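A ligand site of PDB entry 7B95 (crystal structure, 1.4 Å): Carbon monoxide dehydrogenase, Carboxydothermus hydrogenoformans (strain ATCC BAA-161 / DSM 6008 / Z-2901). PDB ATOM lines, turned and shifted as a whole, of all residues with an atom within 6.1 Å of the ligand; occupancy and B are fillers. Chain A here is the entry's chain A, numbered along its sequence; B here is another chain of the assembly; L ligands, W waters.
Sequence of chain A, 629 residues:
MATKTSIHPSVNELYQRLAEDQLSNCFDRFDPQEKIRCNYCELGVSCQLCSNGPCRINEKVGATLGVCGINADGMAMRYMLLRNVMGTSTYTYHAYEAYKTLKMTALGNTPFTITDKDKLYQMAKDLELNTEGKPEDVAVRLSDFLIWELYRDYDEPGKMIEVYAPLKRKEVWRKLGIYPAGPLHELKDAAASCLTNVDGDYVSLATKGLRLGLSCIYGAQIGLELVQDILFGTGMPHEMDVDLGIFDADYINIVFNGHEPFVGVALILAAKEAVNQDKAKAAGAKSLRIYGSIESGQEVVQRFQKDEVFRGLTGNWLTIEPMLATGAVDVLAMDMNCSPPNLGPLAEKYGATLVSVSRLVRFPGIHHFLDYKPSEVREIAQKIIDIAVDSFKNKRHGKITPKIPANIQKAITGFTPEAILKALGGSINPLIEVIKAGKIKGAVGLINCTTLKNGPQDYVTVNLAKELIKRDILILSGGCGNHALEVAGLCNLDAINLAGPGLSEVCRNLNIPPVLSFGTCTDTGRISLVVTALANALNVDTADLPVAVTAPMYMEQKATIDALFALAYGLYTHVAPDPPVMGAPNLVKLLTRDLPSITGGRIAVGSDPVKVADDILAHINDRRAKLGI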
ATOM      1  N   CYS A  47      -1.066 -14.778  10.486  1.00  0.00           N
ATOM      2  CA  CYS A  47      -1.059 -13.356  10.187  1.00  0.00           C
ATOM      3  C   CYS A  47       0.384 -12.863  10.141  1.00  0.00           C
ATOM      4  O   CYS A  47       1.210 -13.183  11.008  1.00  0.00           O
ATOM      5  CB  CYS A  47      -1.807 -12.572  11.253  1.00  0.00           C
ATOM      6  SG  CYS A  47      -2.012 -10.816  10.879  1.00  0.00           S
ATOM      7  N   GLN A  48       0.671 -12.046   9.125  1.00  0.00           N
ATOM      8  CA  GLN A  48       2.005 -11.461   8.936  1.00  0.00           C
ATOM      9  C   GLN A  48       1.958  -9.949   8.800  1.00  0.00           C
ATOM     10  O   GLN A  48       2.830  -9.342   8.174  1.00  0.00           O
ATOM     11  CB  GLN A  48       2.730 -12.064   7.753  1.00  0.00           C
ATOM     12  CG  GLN A  48       2.740 -13.563   7.699  1.00  0.00           C
ATOM     13  CD  GLN A  48       1.454 -14.201   7.229  1.00  0.00           C
ATOM     14  OE1 GLN A  48       0.690 -13.637   6.445  1.00  0.00           O
ATOM     15  NE2 GLN A  48       1.210 -15.407   7.713  1.00  0.00           N
ATOM     16  N   LEU A  49       0.964  -9.316   9.409  1.00  0.00           N
ATOM     17  CA  LEU A  49       0.716  -7.902   9.135  1.00  0.00           C
ATOM     18  C   LEU A  49       1.511  -6.919   9.992  1.00  0.00           C
ATOM     19  O   LEU A  49       1.517  -5.721   9.667  1.00  0.00           O
ATOM     20  CB  LEU A  49      -0.781  -7.565   9.196  1.00  0.00           C
ATOM     21  CG  LEU A  49      -1.630  -8.284   8.136  1.00  0.00           C
ATOM     22  CD1 LEU A  49      -3.038  -7.718   8.106  1.00  0.00           C
ATOM     23  CD2 LEU A  49      -1.034  -8.266   6.729  1.00  0.00           C
ATOM     24  N   CYS A  50       2.134  -7.355  11.085  1.00  0.00           N
ATOM     25  CA  CYS A  50       2.976  -6.417  11.830  1.00  0.00           C
ATOM     26  C   CYS A  50       4.149  -7.146  12.456  1.00  0.00           C
ATOM     27  O   CYS A  50       4.253  -8.372  12.417  1.00  0.00           O
ATOM     28  CB  CYS A  50       2.208  -5.632  12.885  1.00  0.00           C
ATOM     29  SG  CYS A  50       1.942  -6.533  14.450  1.00  0.00           S
ATOM     30  N   SER A  51       5.065  -6.358  13.028  1.00  0.00           N
ATOM     31  CA  SER A  51       6.302  -6.929  13.532  1.00  0.00           C
ATOM     32  C   SER A  51       6.136  -7.809  14.759  1.00  0.00           C
ATOM     33  O   SER A  51       7.063  -8.560  15.076  1.00  0.00           O
ATOM     34  CB  SER A  51       7.349  -5.850  13.840  1.00  0.00           C
ATOM     35  OG  SER A  51       6.972  -5.120  14.990  1.00  0.00           O
ATOM     36  N   ASN A  52       5.017  -7.721  15.489  1.00  0.00           N
ATOM     37  CA  ASN A  52       4.796  -8.659  16.597  1.00  0.00           C
ATOM     38  C   ASN A  52       4.506 -10.074  16.119  1.00  0.00           C
ATOM     39  O   ASN A  52       4.559 -11.027  16.921  1.00  0.00           O
ATOM     40  CB  ASN A  52       3.665  -8.191  17.504  1.00  0.00           C
ATOM     41  CG  ASN A  52       4.080  -7.078  18.461  1.00  0.00           C
ATOM     42  OD1 ASN A  52       5.064  -7.184  19.162  1.00  0.00           O
ATOM     43  ND2 ASN A  52       3.320  -6.011  18.480  1.00  0.00           N
ATOM     44  N   GLY A  53       4.192 -10.228  14.852  1.00  0.00           N
ATOM     45  CA  GLY A  53       4.003 -11.513  14.239  1.00  0.00           C
ATOM     46  C   GLY A  53       5.327 -12.167  13.887  1.00  0.00           C
ATOM     47  O   GLY A  53       6.400 -11.745  14.328  1.00  0.00           O
ATOM     48  N   PRO A  54       5.258 -13.236  13.085  1.00  0.00           N
ATOM     49  CA  PRO A  54       4.040 -13.799  12.489  1.00  0.00           C
ATOM     50  C   PRO A  54       3.245 -14.470  13.581  1.00  0.00           C
ATOM     51  O   PRO A  54       3.803 -15.168  14.459  1.00  0.00           O
ATOM     52  CB  PRO A  54       4.603 -14.806  11.494  1.00  0.00           C
ATOM     53  CG  PRO A  54       5.967 -15.210  12.054  1.00  0.00           C
ATOM     54  CD  PRO A  54       6.482 -13.963  12.705  1.00  0.00           C
ATOM     55  N   CYS A  55       1.926 -14.304  13.514  1.00  0.00           N
ATOM     56  CA  CYS A  55       1.039 -14.867  14.530  1.00  0.00           C
ATOM     57  C   CYS A  55       0.251 -16.026  13.955  1.00  0.00           C
ATOM     58  O   CYS A  55       0.006 -16.111  12.757  1.00  0.00           O
ATOM     59  CB  CYS A  55       0.045 -13.822  15.064  1.00  0.00           C
ATOM     60  SG  CYS A  55       0.844 -12.565  16.128  1.00  0.00           S
ATOM     61  N   LEU A  65      -5.514 -15.639  20.557  1.00  0.00           N
ATOM     62  CA  LEU A  65      -5.584 -14.350  19.887  1.00  0.00           C
ATOM     63  C   LEU A  65      -4.183 -14.012  19.384  1.00  0.00           C
ATOM     64  O   LEU A  65      -3.177 -14.464  19.928  1.00  0.00           O
ATOM     65  CB  LEU A  65      -6.038 -13.261  20.869  1.00  0.00           C
ATOM     66  CG  LEU A  65      -7.418 -13.421  21.527  1.00  0.00           C
ATOM     67  CD1 LEU A  65      -7.606 -12.318  22.530  1.00  0.00           C
ATOM     68  CD2 LEU A  65      -8.530 -13.421  20.496  1.00  0.00           C
ATOM     69  N   GLY A  66      -4.114 -13.158  18.359  1.00  0.00           N
ATOM     70  CA  GLY A  66      -2.844 -12.555  17.965  1.00  0.00           C
ATOM     71  C   GLY A  66      -2.307 -11.635  19.047  1.00  0.00           C
ATOM     72  O   GLY A  66      -2.990 -11.307  20.002  1.00  0.00           O
ATOM     73  N   VAL A  67      -1.029 -11.238  18.924  1.00  0.00           N
ATOM     74  CA  VAL A  67      -0.452 -10.408  19.997  1.00  0.00           C
ATOM     75  C   VAL A  67      -1.284  -9.152  20.204  1.00  0.00           C
ATOM     76  O   VAL A  67      -1.535  -8.747  21.356  1.00  0.00           O
ATOM     77  CB  VAL A  67       1.023 -10.067  19.701  1.00  0.00           C
ATOM     78  CG1 VAL A  67       1.588  -9.123  20.748  1.00  0.00           C
ATOM     79  CG2 VAL A  67       1.827 -11.305  19.644  1.00  0.00           C
ATOM     80  N   CYS A  68      -1.763  -8.543  19.106  1.00  0.00           N
ATOM     81  CA  CYS A  68      -2.556  -7.317  19.178  1.00  0.00           C
ATOM     82  C   CYS A  68      -3.936  -7.534  19.790  1.00  0.00           C
ATOM     83  O   CYS A  68      -4.603  -6.552  20.117  1.00  0.00           O
ATOM     84  CB  CYS A  68      -2.743  -6.776  17.776  1.00  0.00           C
ATOM     85  SG  CYS A  68      -3.587  -7.945  16.644  1.00  0.00           S
ATOM     86  N   GLY A  69      -4.419  -8.777  19.865  1.00  0.00           N
ATOM     87  CA  GLY A  69      -5.743  -9.062  20.398  1.00  0.00           C
ATOM     88  C   GLY A  69      -6.758  -9.564  19.381  1.00  0.00           C
ATOM     89  O   GLY A  69      -7.869  -9.886  19.785  1.00  0.00           O
ATOM     90  N   ILE A  70      -6.431  -9.640  18.094  1.00  0.00           N
ATOM     91  CA  ILE A  70      -7.428 -10.027  17.096  1.00  0.00           C
ATOM     92  C   ILE A  70      -7.712 -11.521  17.210  1.00  0.00           C
ATOM     93  O   ILE A  70      -6.821 -12.319  17.524  1.00  0.00           O
ATOM     94  CB  ILE A  70      -6.957  -9.630  15.697  1.00  0.00           C
ATOM     95  CG1 ILE A  70      -8.163  -9.577  14.728  1.00  0.00           C
ATOM     96  CG2 ILE A  70      -5.858 -10.530  15.186  1.00  0.00           C
ATOM     97  CD1 ILE A  70      -7.796  -8.991  13.388  1.00  0.00           C
ATOM     98  N   MET A  75      -8.901 -12.109  11.947  1.00  0.00           N
ATOM     99  CA  MET A  75      -7.677 -12.377  11.225  1.00  0.00           C
ATOM    100  C   MET A  75      -7.959 -12.858   9.802  1.00  0.00           C
ATOM    101  O   MET A  75      -7.401 -12.336   8.827  1.00  0.00           O
ATOM    102  CB  MET A  75      -6.870 -13.405  12.005  1.00  0.00           C
ATOM    103  CG  MET A  75      -5.547 -13.798  11.406  1.00  0.00           C
ATOM    104  SD  MET A  75      -4.611 -15.006  12.369  1.00  0.00           S
ATOM    105  CE  MET A  75      -4.302 -14.089  13.829  1.00  0.00           C
ATOM    106  N   ARG A  78      -9.801 -10.249   7.586  1.00  0.00           N
ATOM    107  CA  ARG A  78      -8.957  -9.104   7.263  1.00  0.00           C
ATOM    108  C   ARG A  78      -7.999  -9.421   6.123  1.00  0.00           C
ATOM    109  O   ARG A  78      -7.815  -8.600   5.218  1.00  0.00           O
ATOM    110  CB  ARG A  78      -8.185  -8.641   8.499  1.00  0.00           C
ATOM    111  CG  ARG A  78      -7.257  -7.484   8.256  1.00  0.00           C
ATOM    112  CD  ARG A  78      -6.692  -6.957   9.550  1.00  0.00           C
ATOM    113  NE  ARG A  78      -5.885  -7.969  10.199  1.00  0.00           N
ATOM    114  CZ  ARG A  78      -5.243  -7.795  11.342  1.00  0.00           C
ATOM    115  NH1 ARG A  78      -5.304  -6.633  11.989  1.00  0.00           N
ATOM    116  NH2 ARG A  78      -4.525  -8.791  11.844  1.00  0.00           N
ATOM    117  N   THR A 196      -2.820  -3.000  11.053  1.00  0.00           N
ATOM    118  CA  THR A 196      -2.927  -3.475  12.435  1.00  0.00           C
ATOM    119  C   THR A 196      -3.588  -2.430  13.335  1.00  0.00           C
ATOM    120  O   THR A 196      -3.365  -1.212  13.213  1.00  0.00           O
ATOM    121  CB  THR A 196      -1.530  -3.795  12.937  1.00  0.00           C
ATOM    122  OG1 THR A 196      -0.914  -4.753  12.056  1.00  0.00           O
ATOM    123  CG2 THR A 196      -1.521  -4.319  14.384  1.00  0.00           C
ATOM    124  N   ASN A 197      -4.468  -2.922  14.222  1.00  0.00           N
ATOM    125  CA  ASN A 197      -5.145  -2.099  15.224  1.00  0.00           C
ATOM    126  C   ASN A 197      -6.062  -1.038  14.612  1.00  0.00           C
ATOM    127  O   ASN A 197      -6.262   0.027  15.209  1.00  0.00           O
ATOM    128  CB  ASN A 197      -4.153  -1.473  16.225  1.00  0.00           C
ATOM    129  CG  ASN A 197      -3.432  -2.495  17.041  1.00  0.00           C
ATOM    130  OD1 ASN A 197      -3.967  -3.583  17.329  1.00  0.00           O
ATOM    131  ND2 ASN A 197      -2.193  -2.174  17.445  1.00  0.00           N
ATOM    132  N   ARG B  37       6.245 -20.227  16.406  1.00  0.00           N
ATOM    133  CA  ARG B  37       6.577 -19.254  15.367  1.00  0.00           C
ATOM    134  C   ARG B  37       6.971 -19.920  14.054  1.00  0.00           C
ATOM    135  O   ARG B  37       7.677 -20.924  14.015  1.00  0.00           O
ATOM    136  CB  ARG B  37       7.732 -18.335  15.791  1.00  0.00           C
ATOM    137  CG  ARG B  37       7.436 -17.373  16.932  1.00  0.00           C
ATOM    138  CD  ARG B  37       6.386 -16.318  16.607  1.00  0.00           C
ATOM    139  NE  ARG B  37       6.443 -15.311  17.649  1.00  0.00           N
ATOM    140  CZ  ARG B  37       5.773 -14.160  17.620  1.00  0.00           C
ATOM    141  NH1 ARG B  37       5.928 -13.273  18.589  1.00  0.00           N
ATOM    142  NH2 ARG B  37       4.921 -13.908  16.636  1.00  0.00           N
ATOM    143  N   MET B 555       6.533  -1.266  13.996  1.00  0.00           N
ATOM    144  CA  MET B 555       5.426  -2.204  14.139  1.00  0.00           C
ATOM    145  C   MET B 555       4.673  -2.394  12.835  1.00  0.00           C
ATOM    146  O   MET B 555       4.513  -3.518  12.364  1.00  0.00           O
ATOM    147  CB  MET B 555       4.463  -1.746  15.244  1.00  0.00           C
ATOM    148  CG  MET B 555       3.480  -2.852  15.719  1.00  0.00           C
ATOM    149  SD  MET B 555       1.910  -2.864  14.995  1.00  0.00           S
ATOM    150  CE  MET B 555       1.181  -1.438  15.826  1.00  0.00           C
HETATM  151 FE1  LIG L   1       0.038 -10.697  15.068  1.00  0.00          FE
HETATM  152 FE2  LIG L   1       0.453  -8.209  14.109  1.00  0.00          FE
HETATM  153 FE3  LIG L   1      -1.972  -8.813  15.263  1.00  0.00          FE
HETATM  154 FE4  LIG L   1      -1.225  -9.913  12.837  1.00  0.00          FE
HETATM  155  S1  LIG L   1      -1.644  -7.701  13.236  1.00  0.00           S
HETATM  156  S2  LIG L   1      -2.233 -10.998  14.616  1.00  0.00           S
HETATM  157  S3  LIG L   1       1.040 -10.150  13.065  1.00  0.00           S
HETATM  158  S4  LIG L   1       0.081  -8.811  16.330  1.00  0.00           S
HETATM  159  O   HOH W   1       0.774  -5.542  17.353  1.00  0.00           O
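S1 of the ligand lies close to NH2 of Arg 78, 3.4 Å away. An iron atom (FE3) of the ligand is bound by the side-chain sulfur of Cys 68 (2.3 Å). A sulfur (S3) of the ligand sits close to the backbone NH (N) of Gly 53, at 3.6 Å. The backbone NH of Cys 50 sits close to a sulfur (S3) of the ligand (3.6 Å). A sulfur (S1) of the ligand lies close to the side-chain hydroxyl (OG1) of Thr 196 (3.3 Å). N of Cys 68 sits close to S4 of the ligand, 3.3 Å away. SG of Cys 47 binds FE4 of the ligand (2.3 Å). The backbone NH of Leu 49 sits close to a sulfur (S3) of the ligand, at 3.8 Å. A sulfur (S4) of the ligand sits close to the backbone NH (N) of Val 67 (3.7 Å). The side-chain sulfur of Cys 50 is bound to an iron atom (FE2) of the ligand (2.3 Å). SG of Cys 55 binds FE1 of the ligand (2.3 Å).
The backbone carbonyl oxygen of Gly 53 sits close to the guanidinium group of Arg 37 of chain B. N of Cys 55 sits at hydrogen-bond distance from O of Cys 47, 2.8 Å away. SG of Cys 55 sits close to N of Val 67 (3.6 Å). The side-chain sulfur (SG) of Cys 68 lies close to the backbone NH (N) of Ile 70 (3.6 Å). SG of Cys 47 lies close to N of Leu 49, 3.6 Å away. The side-chain sulfur of Cys 50 sits close to the side-chain sulfur of Met 555 of chain B (3.7 Å). The backbone NH (N) of Asn 52 lies close to the side-chain sulfur (SG) of Cys 50 (3.5 Å). NH2 of Arg 78 sits close to SG of Cys 47.
Residues that only touch the ligand: Ile 70, Gly 66, Met 75 and Asn 52. Hydrophobic or aromatic side chains within 4 Å of the ligand: Val 67, Ile 70 and Met 75. 13 residues have an atom within 4 Å of the ligand: Cys 47, Leu 49, Cys 50, Asn 52, Gly 53, Cys 55, Gly 66, Val 67, Cys 68, Ile 70, Met 75, Arg 78 and Thr 196. Along chain A the residues within 4 Å of the ligand span positions 47 to 196. The nearest printed residue that does not touch the ligand is Gln 48 (4.4 Å).
Water W1 lies within hydrogen-bond range of the side-chain amide nitrogen (ND2) of Asn 52, a sulfur (S4) of the ligand and the side-chain sulfur (SD) of Met 555 of chain B.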
